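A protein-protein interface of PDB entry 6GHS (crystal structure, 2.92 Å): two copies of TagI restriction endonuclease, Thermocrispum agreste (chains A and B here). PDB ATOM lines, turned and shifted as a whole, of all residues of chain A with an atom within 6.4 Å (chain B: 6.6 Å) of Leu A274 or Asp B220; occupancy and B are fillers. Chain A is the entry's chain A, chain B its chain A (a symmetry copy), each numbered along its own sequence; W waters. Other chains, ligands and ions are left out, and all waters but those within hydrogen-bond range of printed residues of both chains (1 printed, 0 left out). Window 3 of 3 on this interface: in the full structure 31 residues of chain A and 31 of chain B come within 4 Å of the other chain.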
ATOM      1  N   ASN A 259     -24.478  -7.191  21.381  1.00  0.00           N
ATOM      2  CA  ASN A 259     -24.840  -7.176  19.948  1.00  0.00           C
ATOM      3  C   ASN A 259     -24.025  -8.134  19.081  1.00  0.00           C
ATOM      4  O   ASN A 259     -23.484  -7.730  18.043  1.00  0.00           O
ATOM      5  CB  ASN A 259     -24.695  -5.760  19.420  1.00  0.00           C
ATOM      6  CG  ASN A 259     -25.543  -4.797  20.183  1.00  0.00           C
ATOM      7  OD1 ASN A 259     -26.753  -4.764  19.999  1.00  0.00           O
ATOM      8  ND2 ASN A 259     -24.927  -4.038  21.081  1.00  0.00           N
ATOM      9  N   GLY A 260     -23.943  -9.391  19.526  1.00  0.00           N
ATOM     10  CA  GLY A 260     -23.362 -10.499  18.754  1.00  0.00           C
ATOM     11  C   GLY A 260     -21.907 -10.422  18.298  1.00  0.00           C
ATOM     12  O   GLY A 260     -21.584 -10.963  17.236  1.00  0.00           O
ATOM     13  N   ALA A 261     -21.035  -9.757  19.061  1.00  0.00           N
ATOM     14  CA  ALA A 261     -19.595  -9.652  18.705  1.00  0.00           C
ATOM     15  C   ALA A 261     -18.628 -10.426  19.647  1.00  0.00           C
ATOM     16  O   ALA A 261     -17.412 -10.494  19.399  1.00  0.00           O
ATOM     17  CB  ALA A 261     -19.201  -8.185  18.610  1.00  0.00           C
ATOM     18  N   LEU A 262     -19.180 -10.998  20.719  1.00  0.00           N
ATOM     19  CA  LEU A 262     -18.451 -11.812  21.675  1.00  0.00           C
ATOM     20  C   LEU A 262     -19.365 -12.948  22.126  1.00  0.00           C
ATOM     21  O   LEU A 262     -20.578 -12.771  22.239  1.00  0.00           O
ATOM     22  CB  LEU A 262     -18.084 -10.981  22.895  1.00  0.00           C
ATOM     23  CG  LEU A 262     -17.145  -9.802  22.665  1.00  0.00           C
ATOM     24  CD1 LEU A 262     -17.159  -8.849  23.860  1.00  0.00           C
ATOM     25  CD2 LEU A 262     -15.736 -10.292  22.338  1.00  0.00           C
ATOM     26  N   VAL A 271     -14.534 -15.395  22.814  1.00  0.00           N
ATOM     27  CA  VAL A 271     -14.364 -15.643  21.391  1.00  0.00           C
ATOM     28  C   VAL A 271     -15.040 -14.553  20.598  1.00  0.00           C
ATOM     29  O   VAL A 271     -16.164 -14.188  20.911  1.00  0.00           O
ATOM     30  CB  VAL A 271     -15.025 -16.960  20.977  1.00  0.00           C
ATOM     31  CG1 VAL A 271     -14.593 -17.343  19.562  1.00  0.00           C
ATOM     32  CG2 VAL A 271     -14.704 -18.057  21.985  1.00  0.00           C
ATOM     33  N   ASN A 272     -14.369 -14.065  19.555  1.00  0.00           N
ATOM     34  CA  ASN A 272     -14.944 -13.078  18.637  1.00  0.00           C
ATOM     35  C   ASN A 272     -15.991 -13.761  17.751  1.00  0.00           C
ATOM     36  O   ASN A 272     -15.658 -14.503  16.832  1.00  0.00           O
ATOM     37  CB  ASN A 272     -13.835 -12.451  17.786  1.00  0.00           C
ATOM     38  CG  ASN A 272     -14.324 -11.324  16.868  1.00  0.00           C
ATOM     39  OD1 ASN A 272     -15.445 -11.328  16.349  1.00  0.00           O
ATOM     40  ND2 ASN A 272     -13.450 -10.356  16.646  1.00  0.00           N
ATOM     41  N   ALA A 273     -17.257 -13.484  18.025  1.00  0.00           N
ATOM     42  CA  ALA A 273     -18.357 -14.058  17.263  1.00  0.00           C
ATOM     43  C   ALA A 273     -18.401 -13.666  15.773  1.00  0.00           C
ATOM     44  O   ALA A 273     -18.983 -14.387  14.968  1.00  0.00           O
ATOM     45  CB  ALA A 273     -19.676 -13.709  17.931  1.00  0.00           C
ATOM     46  N   LEU A 274     -17.809 -12.540  15.398  1.00  0.00           N
ATOM     47  CA  LEU A 274     -17.868 -12.098  14.012  1.00  0.00           C
ATOM     48  C   LEU A 274     -16.979 -12.924  13.110  1.00  0.00           C
ATOM     49  O   LEU A 274     -17.374 -13.260  11.994  1.00  0.00           O
ATOM     50  CB  LEU A 274     -17.479 -10.622  13.876  1.00  0.00           C
ATOM     51  CG  LEU A 274     -18.292  -9.576  14.652  1.00  0.00           C
ATOM     52  CD1 LEU A 274     -17.807  -8.170  14.310  1.00  0.00           C
ATOM     53  CD2 LEU A 274     -19.786  -9.707  14.400  1.00  0.00           C
ATOM     54  N   ASN A 275     -15.776 -13.232  13.578  1.00  0.00           N
ATOM     55  CA  ASN A 275     -14.811 -13.968  12.756  1.00  0.00           C
ATOM     56  C   ASN A 275     -14.390 -15.332  13.315  1.00  0.00           C
ATOM     57  O   ASN A 275     -13.577 -16.005  12.686  1.00  0.00           O
ATOM     58  CB  ASN A 275     -13.577 -13.096  12.469  1.00  0.00           C
ATOM     59  CG  ASN A 275     -12.792 -12.755  13.714  1.00  0.00           C
ATOM     60  OD1 ASN A 275     -12.941 -13.391  14.747  1.00  0.00           O
ATOM     61  ND2 ASN A 275     -11.952 -11.745  13.620  1.00  0.00           N
ATOM     62  N   GLY A 276     -14.917 -15.725  14.479  1.00  0.00           N
ATOM     63  CA  GLY A 276     -14.580 -17.012  15.114  1.00  0.00           C
ATOM     64  C   GLY A 276     -13.292 -17.062  15.928  1.00  0.00           C
ATOM     65  O   GLY A 276     -13.061 -18.022  16.672  1.00  0.00           O
ATOM     66  N   GLU A 277     -12.468 -16.021  15.810  1.00  0.00           N
ATOM     67  CA  GLU A 277     -11.150 -15.985  16.427  1.00  0.00           C
ATOM     68  C   GLU A 277     -11.265 -15.927  17.953  1.00  0.00           C
ATOM     69  O   GLU A 277     -12.094 -15.193  18.492  1.00  0.00           O
ATOM     70  CB  GLU A 277     -10.364 -14.783  15.894  1.00  0.00           C
ATOM     71  CG  GLU A 277      -8.888 -14.791  16.274  1.00  0.00           C
ATOM     72  CD  GLU A 277      -7.979 -14.136  15.240  1.00  0.00           C
ATOM     73  OE1 GLU A 277      -6.937 -13.567  15.649  1.00  0.00           O
ATOM     74  OE2 GLU A 277      -8.291 -14.196  14.022  1.00  0.00           O
ATOM     75  N   PRO A 303     -26.694 -15.907  15.397  1.00  0.00           N
ATOM     76  CA  PRO A 303     -27.380 -16.455  14.228  1.00  0.00           C
ATOM     77  C   PRO A 303     -27.160 -17.956  14.005  1.00  0.00           C
ATOM     78  O   PRO A 303     -28.142 -18.702  13.885  1.00  0.00           O
ATOM     79  CB  PRO A 303     -26.811 -15.635  13.065  1.00  0.00           C
ATOM     80  CG  PRO A 303     -26.286 -14.392  13.689  1.00  0.00           C
ATOM     81  CD  PRO A 303     -25.758 -14.838  15.010  1.00  0.00           C
ATOM     82  N   LEU B  86     -28.912 -10.789   8.709  1.00  0.00           N
ATOM     83  CA  LEU B  86     -28.859  -9.333   8.801  1.00  0.00           C
ATOM     84  C   LEU B  86     -28.447  -8.646   7.501  1.00  0.00           C
ATOM     85  O   LEU B  86     -28.138  -7.451   7.511  1.00  0.00           O
ATOM     86  CB  LEU B  86     -27.935  -8.918   9.939  1.00  0.00           C
ATOM     87  CG  LEU B  86     -28.408  -9.401  11.307  1.00  0.00           C
ATOM     88  CD1 LEU B  86     -27.357  -9.093  12.360  1.00  0.00           C
ATOM     89  CD2 LEU B  86     -29.752  -8.790  11.686  1.00  0.00           C
ATOM     90  N   VAL B  95     -31.713  -3.020  13.579  1.00  0.00           N
ATOM     91  CA  VAL B  95     -30.587  -3.057  14.515  1.00  0.00           C
ATOM     92  C   VAL B  95     -29.906  -1.697  14.536  1.00  0.00           C
ATOM     93  O   VAL B  95     -29.502  -1.211  15.587  1.00  0.00           O
ATOM     94  CB  VAL B  95     -29.531  -4.122  14.146  1.00  0.00           C
ATOM     95  CG1 VAL B  95     -28.355  -4.067  15.120  1.00  0.00           C
ATOM     96  CG2 VAL B  95     -30.152  -5.518  14.130  1.00  0.00           C
ATOM     97  N   LEU B  99     -29.058   0.777  17.657  1.00  0.00           N
ATOM     98  CA  LEU B  99     -27.740   1.343  17.954  1.00  0.00           C
ATOM     99  C   LEU B  99     -27.675   2.878  17.931  1.00  0.00           C
ATOM    100  O   LEU B  99     -27.054   3.483  18.811  1.00  0.00           O
ATOM    101  CB  LEU B  99     -26.691   0.794  16.996  1.00  0.00           C
ATOM    102  CG  LEU B  99     -26.444  -0.712  17.060  1.00  0.00           C
ATOM    103  CD1 LEU B  99     -25.370  -1.074  16.039  1.00  0.00           C
ATOM    104  CD2 LEU B  99     -26.064  -1.207  18.451  1.00  0.00           C
ATOM    105  N   HIS B 133     -31.801  -7.111  20.277  1.00  0.00           N
ATOM    106  CA  HIS B 133     -32.142  -8.066  19.227  1.00  0.00           C
ATOM    107  C   HIS B 133     -31.426  -9.394  19.408  1.00  0.00           C
ATOM    108  O   HIS B 133     -30.376  -9.462  20.021  1.00  0.00           O
ATOM    109  CB  HIS B 133     -31.804  -7.492  17.864  1.00  0.00           C
ATOM    110  CG  HIS B 133     -30.339  -7.348  17.630  1.00  0.00           C
ATOM    111  ND1 HIS B 133     -29.672  -6.158  17.816  1.00  0.00           N
ATOM    112  CD2 HIS B 133     -29.404  -8.249  17.246  1.00  0.00           C
ATOM    113  CE1 HIS B 133     -28.389  -6.328  17.540  1.00  0.00           C
ATOM    114  NE2 HIS B 133     -28.202  -7.587  17.189  1.00  0.00           N
ATOM    115  N   PHE B 135     -31.453 -13.899  17.837  1.00  0.00           N
ATOM    116  CA  PHE B 135     -32.007 -14.955  16.999  1.00  0.00           C
ATOM    117  C   PHE B 135     -32.589 -16.041  17.870  1.00  0.00           C
ATOM    118  O   PHE B 135     -32.063 -16.328  18.951  1.00  0.00           O
ATOM    119  CB  PHE B 135     -30.949 -15.511  16.066  1.00  0.00           C
ATOM    120  CG  PHE B 135     -30.596 -14.565  14.974  1.00  0.00           C
ATOM    121  CD1 PHE B 135     -29.777 -13.472  15.230  1.00  0.00           C
ATOM    122  CD2 PHE B 135     -31.120 -14.724  13.705  1.00  0.00           C
ATOM    123  CE1 PHE B 135     -29.462 -12.571  14.226  1.00  0.00           C
ATOM    124  CE2 PHE B 135     -30.808 -13.830  12.699  1.00  0.00           C
ATOM    125  CZ  PHE B 135     -29.979 -12.751  12.958  1.00  0.00           C
ATOM    126  N   GLU B 218     -16.854  -2.814  16.025  1.00  0.00           N
ATOM    127  CA  GLU B 218     -17.598  -3.623  15.073  1.00  0.00           C
ATOM    128  C   GLU B 218     -18.580  -4.489  15.846  1.00  0.00           C
ATOM    129  O   GLU B 218     -18.184  -5.223  16.740  1.00  0.00           O
ATOM    130  CB  GLU B 218     -16.647  -4.490  14.229  1.00  0.00           C
ATOM    131  CG  GLU B 218     -16.056  -3.811  12.979  1.00  0.00           C
ATOM    132  CD  GLU B 218     -17.038  -3.718  11.794  1.00  0.00           C
ATOM    133  OE1 GLU B 218     -17.862  -4.657  11.589  1.00  0.00           O
ATOM    134  OE2 GLU B 218     -16.988  -2.703  11.050  1.00  0.00           O
ATOM    135  N   VAL B 219     -19.859  -4.385  15.509  1.00  0.00           N
ATOM    136  CA  VAL B 219     -20.887  -5.292  16.029  1.00  0.00           C
ATOM    137  C   VAL B 219     -21.490  -6.108  14.867  1.00  0.00           C
ATOM    138  O   VAL B 219     -21.002  -6.019  13.716  1.00  0.00           O
ATOM    139  CB  VAL B 219     -21.958  -4.536  16.868  1.00  0.00           C
ATOM    140  CG1 VAL B 219     -21.308  -3.832  18.045  1.00  0.00           C
ATOM    141  CG2 VAL B 219     -22.743  -3.524  16.046  1.00  0.00           C
ATOM    142  N   ASP B 220     -22.518  -6.911  15.167  1.00  0.00           N
ATOM    143  CA  ASP B 220     -23.092  -7.837  14.179  1.00  0.00           C
ATOM    144  C   ASP B 220     -23.524  -7.163  12.897  1.00  0.00           C
ATOM    145  O   ASP B 220     -23.178  -7.620  11.824  1.00  0.00           O
ATOM    146  CB  ASP B 220     -24.232  -8.712  14.750  1.00  0.00           C
ATOM    147  CG  ASP B 220     -25.398  -7.910  15.340  1.00  0.00           C
ATOM    148  OD1 ASP B 220     -25.306  -6.683  15.488  1.00  0.00           O
ATOM    149  OD2 ASP B 220     -26.420  -8.533  15.675  1.00  0.00           O
ATOM    150  N   VAL B 221     -24.243  -6.061  13.009  1.00  0.00           N
ATOM    151  CA  VAL B 221     -24.747  -5.377  11.829  1.00  0.00           C
ATOM    152  C   VAL B 221     -23.713  -4.500  11.122  1.00  0.00           C
ATOM    153  O   VAL B 221     -23.873  -4.210   9.943  1.00  0.00           O
ATOM    154  CB  VAL B 221     -26.030  -4.568  12.147  1.00  0.00           C
ATOM    155  CG1 VAL B 221     -25.733  -3.301  12.937  1.00  0.00           C
ATOM    156  CG2 VAL B 221     -26.780  -4.220  10.867  1.00  0.00           C
ATOM    157  N   GLY B 222     -22.668  -4.073  11.825  1.00  0.00           N
ATOM    158  CA  GLY B 222     -21.695  -3.165  11.236  1.00  0.00           C
ATOM    159  C   GLY B 222     -20.968  -2.331  12.263  1.00  0.00           C
ATOM    160  O   GLY B 222     -20.854  -2.773  13.393  1.00  0.00           O
HETATM  161  O   HOH W   1     -29.008  -6.185  21.312  1.00  0.00           O
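OD1 of Asn A259 touches CD2 of Leu B99, at 3.9 Å.
Asn A259 touches His B133 (OD1 to CE1, 3.3 Å).
O of Asn A259 touches CB of Val B219, at 3.7 Å.
CB of Ala A261 touches O of Glu B218 (3.6 Å).
Leu A274 touches Glu B218.
Leu A274 touches Val B219 (CD1 to O, 3.9 Å).
Leu A274 touches Asp B220 (CD2 to CA, 3.8 Å).
Pro A303 touches Phe B135 (CG to CE1, 3.7 Å).
No position is printed for both chains.
Of the 10 printed residues of chain B, 6 touch a printed residue of chain A.
Printed residues of chain B that touch a printed residue of chain A: Leu B99, His B133, Phe B135, Glu B218, Val B219 and Asp B220.
Hydrophobic or aromatic side chains of chain B that line the printed part of chain A: Leu B99, His B133, Phe B135 and Val B219.
Of the 12 printed residues of chain A, 4 touch a printed residue of chain B.
Among the printed residues, no Asp or Glu carboxylate lies within 4 Å of a Lys or Arg side-chain nitrogen of the other chain.
Printed residues of chain B within 4 Å of Ala A261: Glu B218.
Ala A273 touches none of the printed residues of chain B.
Leu A274 touches just these residues of chain B: Glu B218 (3.8 Å), Val B219 (3.9 Å) and Asp B220 (3.8 Å).
Of the printed residues of chain B, Pro A303 touches Phe B135.
Of the printed residues of chain A, Leu B99 touches Asn A259 (3.9 Å).
Of the printed residues of chain A, His B133 touches Asn A259.
Of the printed residues of chain A, Val B219 touches Asn A259 and Leu A274.
Val B221 touches none of the printed residues of chain A.
The nearest residue of chain A that does not touch Asp B220 is Gly A260 (4.3 Å).
OD2 of Asp B220 sits at hydrogen-bond distance from NE2 of His B133, at 2.5 Å.
N of Ala A273 sits at hydrogen-bond distance from O of Ala A261, at 3.3 Å.
The backbone NH of Leu A274 lies within hydrogen-bond range of the side-chain amide oxygen of Asn A272, 2.8 Å away.
O of Asn A259 sits at hydrogen-bond distance from N of Asp B220 (3.1 Å).
Water W1 bridges the side-chain amide oxygen (OD1) of Asn A259 and the backbone NH (N) of His B133.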
